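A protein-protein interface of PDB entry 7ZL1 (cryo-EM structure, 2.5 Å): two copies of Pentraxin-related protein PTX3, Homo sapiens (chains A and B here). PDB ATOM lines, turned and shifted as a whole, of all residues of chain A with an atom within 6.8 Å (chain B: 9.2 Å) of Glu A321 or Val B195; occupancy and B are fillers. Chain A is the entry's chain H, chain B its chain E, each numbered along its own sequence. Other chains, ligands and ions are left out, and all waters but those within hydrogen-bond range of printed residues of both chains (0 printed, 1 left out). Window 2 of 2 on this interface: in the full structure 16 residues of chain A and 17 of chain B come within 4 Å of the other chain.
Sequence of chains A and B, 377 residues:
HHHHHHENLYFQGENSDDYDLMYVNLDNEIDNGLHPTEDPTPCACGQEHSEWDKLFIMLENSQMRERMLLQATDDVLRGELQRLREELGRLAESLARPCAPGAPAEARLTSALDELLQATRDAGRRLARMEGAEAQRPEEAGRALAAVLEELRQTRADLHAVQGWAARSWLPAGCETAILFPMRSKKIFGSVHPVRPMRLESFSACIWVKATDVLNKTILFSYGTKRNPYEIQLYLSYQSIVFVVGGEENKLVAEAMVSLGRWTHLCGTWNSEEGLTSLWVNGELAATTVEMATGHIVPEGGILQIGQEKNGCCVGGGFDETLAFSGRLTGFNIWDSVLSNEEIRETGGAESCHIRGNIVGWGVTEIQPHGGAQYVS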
ATOM      1  N   MET A 183      25.853  25.927  -3.363  1.00  0.00           N
ATOM      2  CA  MET A 183      26.510  24.634  -3.354  1.00  0.00           C
ATOM      3  C   MET A 183      27.707  24.725  -4.282  1.00  0.00           C
ATOM      4  O   MET A 183      27.806  25.646  -5.092  1.00  0.00           O
ATOM      5  CB  MET A 183      25.535  23.540  -3.791  1.00  0.00           C
ATOM      6  CG  MET A 183      24.857  23.852  -5.115  1.00  0.00           C
ATOM      7  SD  MET A 183      23.079  23.608  -5.032  1.00  0.00           S
ATOM      8  CE  MET A 183      22.558  24.444  -6.517  1.00  0.00           C
ATOM      9  N   ARG A 184      28.614  23.775  -4.155  1.00  0.00           N
ATOM     10  CA  ARG A 184      29.547  23.496  -5.228  1.00  0.00           C
ATOM     11  C   ARG A 184      28.944  22.470  -6.176  1.00  0.00           C
ATOM     12  O   ARG A 184      28.174  21.598  -5.772  1.00  0.00           O
ATOM     13  CB  ARG A 184      30.900  23.030  -4.681  1.00  0.00           C
ATOM     14  CG  ARG A 184      30.871  21.836  -3.798  1.00  0.00           C
ATOM     15  CD  ARG A 184      32.279  21.330  -3.532  1.00  0.00           C
ATOM     16  NE  ARG A 184      33.010  22.135  -2.571  1.00  0.00           N
ATOM     17  CZ  ARG A 184      33.080  21.873  -1.274  1.00  0.00           C
ATOM     18  NH1 ARG A 184      32.682  20.716  -0.779  1.00  0.00           N
ATOM     19  NH2 ARG A 184      33.626  22.771  -0.461  1.00  0.00           N
ATOM     20  N   SER A 185      29.262  22.608  -7.454  1.00  0.00           N
ATOM     21  CA  SER A 185      28.775  21.677  -8.461  1.00  0.00           C
ATOM     22  C   SER A 185      29.639  21.832  -9.699  1.00  0.00           C
ATOM     23  O   SER A 185      30.502  22.707  -9.776  1.00  0.00           O
ATOM     24  CB  SER A 185      27.287  21.896  -8.781  1.00  0.00           C
ATOM     25  OG  SER A 185      27.089  22.941  -9.707  1.00  0.00           O
ATOM     26  N   LYS A 186      29.415  20.936 -10.654  1.00  0.00           N
ATOM     27  CA  LYS A 186      30.123  20.975 -11.924  1.00  0.00           C
ATOM     28  C   LYS A 186      29.698  22.114 -12.833  1.00  0.00           C
ATOM     29  O   LYS A 186      30.348  22.320 -13.858  1.00  0.00           O
ATOM     30  CB  LYS A 186      29.926  19.649 -12.649  1.00  0.00           C
ATOM     31  CG  LYS A 186      30.823  18.543 -12.123  1.00  0.00           C
ATOM     32  CD  LYS A 186      30.675  17.218 -12.873  1.00  0.00           C
ATOM     33  CE  LYS A 186      29.237  16.852 -13.241  1.00  0.00           C
ATOM     34  NZ  LYS A 186      28.530  16.213 -12.097  1.00  0.00           N
ATOM     35  N   LYS A 187      28.653  22.863 -12.502  1.00  0.00           N
ATOM     36  CA  LYS A 187      28.175  23.901 -13.399  1.00  0.00           C
ATOM     37  C   LYS A 187      27.999  25.286 -12.785  1.00  0.00           C
ATOM     38  O   LYS A 187      27.716  26.221 -13.534  1.00  0.00           O
ATOM     39  CB  LYS A 187      26.855  23.458 -14.044  1.00  0.00           C
ATOM     40  CG  LYS A 187      25.715  23.260 -13.089  1.00  0.00           C
ATOM     41  CD  LYS A 187      24.500  22.718 -13.821  1.00  0.00           C
ATOM     42  CE  LYS A 187      23.309  22.508 -12.887  1.00  0.00           C
ATOM     43  NZ  LYS A 187      22.858  21.081 -12.885  1.00  0.00           N
ATOM     44  N   LEU A 215      37.968  23.446   0.575  1.00  0.00           N
ATOM     45  CA  LEU A 215      38.748  22.264   0.259  1.00  0.00           C
ATOM     46  C   LEU A 215      40.211  22.655   0.051  1.00  0.00           C
ATOM     47  O   LEU A 215      40.641  23.743   0.435  1.00  0.00           O
ATOM     48  CB  LEU A 215      38.167  21.554  -0.965  1.00  0.00           C
ATOM     49  CG  LEU A 215      36.711  21.115  -0.879  1.00  0.00           C
ATOM     50  CD1 LEU A 215      36.275  20.524  -2.202  1.00  0.00           C
ATOM     51  CD2 LEU A 215      36.497  20.144   0.255  1.00  0.00           C
ATOM     52  N   LYS A 217      41.596  23.398  -2.724  1.00  0.00           N
ATOM     53  CA  LYS A 217      41.567  24.533  -3.648  1.00  0.00           C
ATOM     54  C   LYS A 217      40.122  24.957  -3.880  1.00  0.00           C
ATOM     55  O   LYS A 217      39.382  24.244  -4.557  1.00  0.00           O
ATOM     56  CB  LYS A 217      42.225  24.170  -4.975  1.00  0.00           C
ATOM     57  CG  LYS A 217      42.429  25.343  -5.907  1.00  0.00           C
ATOM     58  CD  LYS A 217      43.094  24.912  -7.187  1.00  0.00           C
ATOM     59  CE  LYS A 217      43.679  26.093  -7.924  1.00  0.00           C
ATOM     60  NZ  LYS A 217      43.996  25.762  -9.332  1.00  0.00           N
ATOM     61  N   GLN A 308      34.941  29.867  -9.728  1.00  0.00           N
ATOM     62  CA  GLN A 308      35.303  28.693 -10.509  1.00  0.00           C
ATOM     63  C   GLN A 308      36.436  29.059 -11.452  1.00  0.00           C
ATOM     64  O   GLN A 308      36.640  30.225 -11.789  1.00  0.00           O
ATOM     65  CB  GLN A 308      34.092  28.133 -11.269  1.00  0.00           C
ATOM     66  CG  GLN A 308      34.297  26.793 -11.970  1.00  0.00           C
ATOM     67  CD  GLN A 308      34.923  25.733 -11.098  1.00  0.00           C
ATOM     68  OE1 GLN A 308      36.138  25.659 -10.997  1.00  0.00           O
ATOM     69  NE2 GLN A 308      34.107  24.865 -10.524  1.00  0.00           N
ATOM     70  N   GLY A 318      31.019  20.096 -16.672  1.00  0.00           N
ATOM     71  CA  GLY A 318      32.278  20.447 -17.292  1.00  0.00           C
ATOM     72  C   GLY A 318      33.325  20.964 -16.329  1.00  0.00           C
ATOM     73  O   GLY A 318      34.509  20.664 -16.488  1.00  0.00           O
ATOM     74  N   PHE A 319      32.920  21.739 -15.329  1.00  0.00           N
ATOM     75  CA  PHE A 319      33.881  22.214 -14.348  1.00  0.00           C
ATOM     76  C   PHE A 319      34.212  21.125 -13.336  1.00  0.00           C
ATOM     77  O   PHE A 319      33.457  20.177 -13.132  1.00  0.00           O
ATOM     78  CB  PHE A 319      33.358  23.437 -13.603  1.00  0.00           C
ATOM     79  CG  PHE A 319      33.041  24.597 -14.481  1.00  0.00           C
ATOM     80  CD1 PHE A 319      34.049  25.380 -14.995  1.00  0.00           C
ATOM     81  CD2 PHE A 319      31.736  24.974 -14.701  1.00  0.00           C
ATOM     82  CE1 PHE A 319      33.767  26.464 -15.767  1.00  0.00           C
ATOM     83  CE2 PHE A 319      31.449  26.062 -15.472  1.00  0.00           C
ATOM     84  CZ  PHE A 319      32.467  26.809 -16.006  1.00  0.00           C
ATOM     85  N   ASP A 320      35.365  21.278 -12.696  1.00  0.00           N
ATOM     86  CA  ASP A 320      35.741  20.438 -11.565  1.00  0.00           C
ATOM     87  C   ASP A 320      34.953  20.892 -10.344  1.00  0.00           C
ATOM     88  O   ASP A 320      35.172  21.990  -9.828  1.00  0.00           O
ATOM     89  CB  ASP A 320      37.244  20.533 -11.334  1.00  0.00           C
ATOM     90  CG  ASP A 320      37.758  19.461 -10.420  1.00  0.00           C
ATOM     91  OD1 ASP A 320      36.941  18.718  -9.839  1.00  0.00           O
ATOM     92  OD2 ASP A 320      38.991  19.357 -10.283  1.00  0.00           O
ATOM     93  N   GLU A 321      34.034  20.044  -9.884  1.00  0.00           N
ATOM     94  CA  GLU A 321      33.201  20.386  -8.736  1.00  0.00           C
ATOM     95  C   GLU A 321      34.026  20.663  -7.481  1.00  0.00           C
ATOM     96  O   GLU A 321      33.649  21.518  -6.677  1.00  0.00           O
ATOM     97  CB  GLU A 321      32.190  19.259  -8.504  1.00  0.00           C
ATOM     98  CG  GLU A 321      31.309  19.393  -7.270  1.00  0.00           C
ATOM     99  CD  GLU A 321      31.953  18.866  -6.004  1.00  0.00           C
ATOM    100  OE1 GLU A 321      32.998  18.187  -6.089  1.00  0.00           O
ATOM    101  OE2 GLU A 321      31.399  19.108  -4.918  1.00  0.00           O
ATOM    102  N   THR A 322      35.154  19.971  -7.292  1.00  0.00           N
ATOM    103  CA  THR A 322      35.985  20.205  -6.110  1.00  0.00           C
ATOM    104  C   THR A 322      36.633  21.586  -6.084  1.00  0.00           C
ATOM    105  O   THR A 322      37.029  22.043  -5.010  1.00  0.00           O
ATOM    106  CB  THR A 322      37.071  19.124  -5.970  1.00  0.00           C
ATOM    107  OG1 THR A 322      38.117  19.348  -6.918  1.00  0.00           O
ATOM    108  CG2 THR A 322      36.500  17.724  -6.146  1.00  0.00           C
ATOM    109  N   LEU A 323      36.774  22.254  -7.227  1.00  0.00           N
ATOM    110  CA  LEU A 323      37.340  23.598  -7.252  1.00  0.00           C
ATOM    111  C   LEU A 323      36.332  24.686  -6.904  1.00  0.00           C
ATOM    112  O   LEU A 323      36.740  25.784  -6.528  1.00  0.00           O
ATOM    113  CB  LEU A 323      37.944  23.890  -8.628  1.00  0.00           C
ATOM    114  CG  LEU A 323      38.983  22.873  -9.104  1.00  0.00           C
ATOM    115  CD1 LEU A 323      39.585  23.296 -10.422  1.00  0.00           C
ATOM    116  CD2 LEU A 323      40.066  22.706  -8.060  1.00  0.00           C
ATOM    117  N   ALA A 324      35.037  24.414  -7.028  1.00  0.00           N
ATOM    118  CA  ALA A 324      34.030  25.464  -6.966  1.00  0.00           C
ATOM    119  C   ALA A 324      33.913  26.091  -5.581  1.00  0.00           C
ATOM    120  O   ALA A 324      34.069  25.429  -4.555  1.00  0.00           O
ATOM    121  CB  ALA A 324      32.675  24.908  -7.389  1.00  0.00           C
ATOM    122  N   PHE A 325      33.659  27.393  -5.573  1.00  0.00           N
ATOM    123  CA  PHE A 325      33.289  28.116  -4.370  1.00  0.00           C
ATOM    124  C   PHE A 325      31.877  27.765  -3.923  1.00  0.00           C
ATOM    125  O   PHE A 325      30.991  27.499  -4.735  1.00  0.00           O
ATOM    126  CB  PHE A 325      33.398  29.617  -4.632  1.00  0.00           C
ATOM    127  CG  PHE A 325      33.084  30.468  -3.451  1.00  0.00           C
ATOM    128  CD1 PHE A 325      33.914  30.488  -2.355  1.00  0.00           C
ATOM    129  CD2 PHE A 325      31.952  31.257  -3.443  1.00  0.00           C
ATOM    130  CE1 PHE A 325      33.623  31.275  -1.278  1.00  0.00           C
ATOM    131  CE2 PHE A 325      31.658  32.048  -2.359  1.00  0.00           C
ATOM    132  CZ  PHE A 325      32.496  32.053  -1.275  1.00  0.00           C
ATOM    133  N   VAL B 192      18.866  15.636  -5.185  1.00  0.00           N
ATOM    134  CA  VAL B 192      20.097  15.746  -4.412  1.00  0.00           C
ATOM    135  C   VAL B 192      21.164  14.925  -5.118  1.00  0.00           C
ATOM    136  O   VAL B 192      20.913  13.781  -5.505  1.00  0.00           O
ATOM    137  CB  VAL B 192      19.898  15.261  -2.964  1.00  0.00           C
ATOM    138  CG1 VAL B 192      21.169  15.431  -2.140  1.00  0.00           C
ATOM    139  CG2 VAL B 192      18.740  15.993  -2.311  1.00  0.00           C
ATOM    140  N   HIS B 193      22.356  15.501  -5.277  1.00  0.00           N
ATOM    141  CA  HIS B 193      23.425  14.912  -6.084  1.00  0.00           C
ATOM    142  C   HIS B 193      24.701  14.742  -5.268  1.00  0.00           C
ATOM    143  O   HIS B 193      25.651  15.518  -5.425  1.00  0.00           O
ATOM    144  CB  HIS B 193      23.701  15.768  -7.314  1.00  0.00           C
ATOM    145  CG  HIS B 193      22.501  15.965  -8.175  1.00  0.00           C
ATOM    146  ND1 HIS B 193      22.032  14.990  -9.027  1.00  0.00           N
ATOM    147  CD2 HIS B 193      21.656  17.013  -8.297  1.00  0.00           C
ATOM    148  CE1 HIS B 193      20.956  15.435  -9.648  1.00  0.00           C
ATOM    149  NE2 HIS B 193      20.708  16.660  -9.225  1.00  0.00           N
ATOM    150  N   PRO B 194      24.771  13.719  -4.421  1.00  0.00           N
ATOM    151  CA  PRO B 194      26.028  13.414  -3.725  1.00  0.00           C
ATOM    152  C   PRO B 194      27.167  13.145  -4.697  1.00  0.00           C
ATOM    153  O   PRO B 194      26.996  12.457  -5.703  1.00  0.00           O
ATOM    154  CB  PRO B 194      25.686  12.160  -2.916  1.00  0.00           C
ATOM    155  CG  PRO B 194      24.216  12.106  -2.883  1.00  0.00           C
ATOM    156  CD  PRO B 194      23.736  12.718  -4.136  1.00  0.00           C
ATOM    157  N   VAL B 195      28.349  13.675  -4.385  1.00  0.00           N
ATOM    158  CA  VAL B 195      29.499  13.389  -5.239  1.00  0.00           C
ATOM    159  C   VAL B 195      30.089  12.015  -4.932  1.00  0.00           C
ATOM    160  O   VAL B 195      30.468  11.281  -5.849  1.00  0.00           O
ATOM    161  CB  VAL B 195      30.566  14.497  -5.121  1.00  0.00           C
ATOM    162  CG1 VAL B 195      29.949  15.864  -5.345  1.00  0.00           C
ATOM    163  CG2 VAL B 195      31.292  14.432  -3.798  1.00  0.00           C
ATOM    164  N   ARG B 196      30.172  11.630  -3.656  1.00  0.00           N
ATOM    165  CA  ARG B 196      30.613  10.267  -3.391  1.00  0.00           C
ATOM    166  C   ARG B 196      29.434   9.306  -3.229  1.00  0.00           C
ATOM    167  O   ARG B 196      28.333   9.718  -2.864  1.00  0.00           O
ATOM    168  CB  ARG B 196      31.523  10.224  -2.162  1.00  0.00           C
ATOM    169  CG  ARG B 196      31.025  10.914  -0.923  1.00  0.00           C
ATOM    170  CD  ARG B 196      32.068  10.805   0.191  1.00  0.00           C
ATOM    171  NE  ARG B 196      32.278   9.437   0.658  1.00  0.00           N
ATOM    172  CZ  ARG B 196      32.285   9.062   1.933  1.00  0.00           C
ATOM    173  NH1 ARG B 196      32.238   9.944   2.918  1.00  0.00           N
ATOM    174  NH2 ARG B 196      32.377   7.767   2.229  1.00  0.00           N
ATOM    175  N   PRO B 197      29.652   8.019  -3.505  1.00  0.00           N
ATOM    176  CA  PRO B 197      28.528   7.093  -3.670  1.00  0.00           C
ATOM    177  C   PRO B 197      27.723   6.884  -2.399  1.00  0.00           C
ATOM    178  O   PRO B 197      28.248   6.911  -1.285  1.00  0.00           O
ATOM    179  CB  PRO B 197      29.211   5.787  -4.088  1.00  0.00           C
ATOM    180  CG  PRO B 197      30.531   6.186  -4.578  1.00  0.00           C
ATOM    181  CD  PRO B 197      30.933   7.338  -3.734  1.00  0.00           C
ATOM    182  N   MET B 198      26.430   6.647  -2.593  1.00  0.00           N
ATOM    183  CA  MET B 198      25.487   6.341  -1.525  1.00  0.00           C
ATOM    184  C   MET B 198      25.523   4.879  -1.092  1.00  0.00           C
ATOM    185  O   MET B 198      24.515   4.391  -0.576  1.00  0.00           O
ATOM    186  CB  MET B 198      24.069   6.723  -1.956  1.00  0.00           C
ATOM    187  CG  MET B 198      23.767   8.215  -1.837  1.00  0.00           C
ATOM    188  SD  MET B 198      23.485   8.744  -0.141  1.00  0.00           S
ATOM    189  CE  MET B 198      21.805   8.196   0.123  1.00  0.00           C
ATOM    190  N   GLU B 300      24.707   1.830  -4.221  1.00  0.00           N
ATOM    191  CA  GLU B 300      24.956   3.078  -4.930  1.00  0.00           C
ATOM    192  C   GLU B 300      24.171   3.147  -6.243  1.00  0.00           C
ATOM    193  O   GLU B 300      23.502   2.198  -6.657  1.00  0.00           O
ATOM    194  CB  GLU B 300      26.453   3.260  -5.173  1.00  0.00           C
ATOM    195  CG  GLU B 300      27.066   2.282  -6.157  1.00  0.00           C
ATOM    196  CD  GLU B 300      28.546   2.528  -6.350  1.00  0.00           C
ATOM    197  OE1 GLU B 300      29.279   2.530  -5.339  1.00  0.00           O
ATOM    198  OE2 GLU B 300      28.978   2.727  -7.511  1.00  0.00           O
ATOM    199  N   LEU B 304      18.431  10.134  -5.139  1.00  0.00           N
ATOM    200  CA  LEU B 304      18.032  10.759  -3.881  1.00  0.00           C
ATOM    201  C   LEU B 304      17.189  12.014  -4.120  1.00  0.00           C
ATOM    202  O   LEU B 304      17.603  12.917  -4.845  1.00  0.00           O
ATOM    203  CB  LEU B 304      19.280  11.085  -3.063  1.00  0.00           C
ATOM    204  CG  LEU B 304      19.095  11.725  -1.691  1.00  0.00           C
ATOM    205  CD1 LEU B 304      18.359  10.816  -0.736  1.00  0.00           C
ATOM    206  CD2 LEU B 304      20.452  12.064  -1.140  1.00  0.00           C
ATOM    207  N   GLY B 357      27.007  16.876   6.801  1.00  0.00           N
ATOM    208  CA  GLY B 357      27.343  15.491   6.555  1.00  0.00           C
ATOM    209  C   GLY B 357      28.418  15.293   5.508  1.00  0.00           C
ATOM    210  O   GLY B 357      28.665  16.127   4.645  1.00  0.00           O
ATOM    211  N   ASN B 358      29.085  14.146   5.604  1.00  0.00           N
ATOM    212  CA  ASN B 358      30.124  13.806   4.644  1.00  0.00           C
ATOM    213  C   ASN B 358      29.584  13.151   3.378  1.00  0.00           C
ATOM    214  O   ASN B 358      30.322  13.049   2.398  1.00  0.00           O
ATOM    215  CB  ASN B 358      31.183  12.922   5.308  1.00  0.00           C
ATOM    216  CG  ASN B 358      30.640  11.604   5.789  1.00  0.00           C
ATOM    217  OD1 ASN B 358      29.463  11.306   5.633  1.00  0.00           O
ATOM    218  ND2 ASN B 358      31.501  10.812   6.409  1.00  0.00           N
ATOM    219  N   ILE B 359      28.343  12.670   3.377  1.00  0.00           N
ATOM    220  CA  ILE B 359      27.721  12.172   2.154  1.00  0.00           C
ATOM    221  C   ILE B 359      26.876  13.270   1.511  1.00  0.00           C
ATOM    222  O   ILE B 359      27.093  13.635   0.354  1.00  0.00           O
ATOM    223  CB  ILE B 359      26.879  10.910   2.427  1.00  0.00           C
ATOM    224  CG1 ILE B 359      27.743   9.757   2.952  1.00  0.00           C
ATOM    225  CG2 ILE B 359      26.154  10.463   1.174  1.00  0.00           C
ATOM    226  CD1 ILE B 359      28.852   9.307   1.991  1.00  0.00           C
ATOM    227  N   VAL B 360      25.908  13.803   2.248  1.00  0.00           N
ATOM    228  CA  VAL B 360      25.186  15.001   1.849  1.00  0.00           C
ATOM    229  C   VAL B 360      25.471  16.064   2.892  1.00  0.00           C
ATOM    230  O   VAL B 360      25.227  15.852   4.083  1.00  0.00           O
ATOM    231  CB  VAL B 360      23.673  14.751   1.704  1.00  0.00           C
ATOM    232  CG1 VAL B 360      22.935  16.034   1.351  1.00  0.00           C
ATOM    233  CG2 VAL B 360      23.410  13.705   0.650  1.00  0.00           C
ATOM    234  N   GLY B 361      25.994  17.196   2.449  1.00  0.00           N
ATOM    235  CA  GLY B 361      26.196  18.339   3.309  1.00  0.00           C
ATOM    236  C   GLY B 361      25.356  19.512   2.867  1.00  0.00           C
ATOM    237  O   GLY B 361      25.429  19.922   1.710  1.00  0.00           O
ATOM    238  N   GLY B 363      24.402  23.008   1.914  1.00  0.00           N
ATOM    239  CA  GLY B 363      25.243  24.077   1.428  1.00  0.00           C
ATOM    240  C   GLY B 363      26.457  23.673   0.616  1.00  0.00           C
ATOM    241  O   GLY B 363      27.144  24.557   0.101  1.00  0.00           O
ATOM    242  N   VAL B 364      26.744  22.381   0.469  1.00  0.00           N
ATOM    243  CA  VAL B 364      27.874  21.965  -0.353  1.00  0.00           C
ATOM    244  C   VAL B 364      27.396  20.962  -1.394  1.00  0.00           C
ATOM    245  O   VAL B 364      27.779  21.047  -2.560  1.00  0.00           O
ATOM    246  CB  VAL B 364      29.030  21.397   0.497  1.00  0.00           C
ATOM    247  CG1 VAL B 364      29.292  22.302   1.676  1.00  0.00           C
ATOM    248  CG2 VAL B 364      28.758  19.971   0.950  1.00  0.00           C
ATOM    249  N   THR B 365      26.537  20.030  -0.998  1.00  0.00           N
ATOM    250  CA  THR B 365      25.957  19.104  -1.961  1.00  0.00           C
ATOM    251  C   THR B 365      24.957  19.829  -2.853  1.00  0.00           C
ATOM    252  O   THR B 365      24.114  20.588  -2.376  1.00  0.00           O
ATOM    253  CB  THR B 365      25.281  17.943  -1.246  1.00  0.00           C
ATOM    254  OG1 THR B 365      26.260  17.209  -0.510  1.00  0.00           O
ATOM    255  CG2 THR B 365      24.614  17.026  -2.250  1.00  0.00           C
ATOM    256  N   GLU B 366      25.061  19.600  -4.154  1.00  0.00           N
ATOM    257  CA  GLU B 366      24.113  20.165  -5.100  1.00  0.00           C
ATOM    258  C   GLU B 366      22.695  19.671  -4.823  1.00  0.00           C
ATOM    259  O   GLU B 366      22.432  18.469  -4.856  1.00  0.00           O
ATOM    260  CB  GLU B 366      24.541  19.803  -6.519  1.00  0.00           C
ATOM    261  CG  GLU B 366      23.586  20.266  -7.606  1.00  0.00           C
ATOM    262  CD  GLU B 366      24.026  19.823  -8.989  1.00  0.00           C
ATOM    263  OE1 GLU B 366      24.836  18.885  -9.086  1.00  0.00           O
ATOM    264  OE2 GLU B 366      23.569  20.413  -9.984  1.00  0.00           O
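The backbone carbonyl oxygen (O) of Val B364 sits at hydrogen-bond distance from the backbone NH (N) of Arg A184, 3.3 Å away.
The side-chain amino group (NZ) of Lys A187 is in salt-bridge range of the side-chain carboxylate (OE2) of Glu B366 (3.1 Å).
N of His B193 lies within hydrogen-bond range of O of Glu B366 (3.0 Å).
The side-chain hydroxyl (OG) of Ser A185 sits close to the backbone NH (N) of Lys A187 (3.2 Å).
The backbone NH (N) of Gly B361 is in hydrogen-bond range of the side-chain hydroxyl (OG1) of Thr B365 (3.0 Å).
Met A183 touches Gly B363.
Met A183 touches Val B364.
CB of Met A183 touches O of Thr B365 (3.6 Å).
Glu B366 touches Met A183.
Glu B366 touches Ser A185 (CD to CB, 3.9 Å).
Glu A321 touches Val B195 (OE2 to CG1, 3.6 Å).
Printed residues of chain B within 4 Å of Met A183: Gly B363, Val B364, Thr B365 and Glu B366.
Printed residues of chain B within 4 Å of Ser A185: Glu B366 (3.9 Å).
Of the printed residues of chain B, Lys A187 touches Glu B366 (3.1 Å).
No residue of chain B comes within 4 Å of Asp A320.
Glu A321 touches just one residue of chain B: Val B195.
No residue of chain B comes within 4 Å of Thr A322.
Ala A324 touches none of the printed residues of chain B.
Printed residues of chain A within 4 Å of Val B195: Glu A321 (3.6 Å).
The nearest residue of chain B that does not touch Glu A321 is Val B364 (4.7 Å).
Of the 16 printed residues of chain A, 5 touch a printed residue of chain B.
Hydrophobic or aromatic side chains of chain A that line the printed part of chain B: Met A183.
Of the 18 printed residues of chain B, 5 touch a printed residue of chain A.
Printed residues of chain B that touch a printed residue of chain A: Val B195, Gly B363, Val B364, Thr B365 and Glu B366.
No position is printed for both chains.
Of the 8 pairs that touch across the chains among the printed residues, none has its exchanged pair printed and touching as well.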
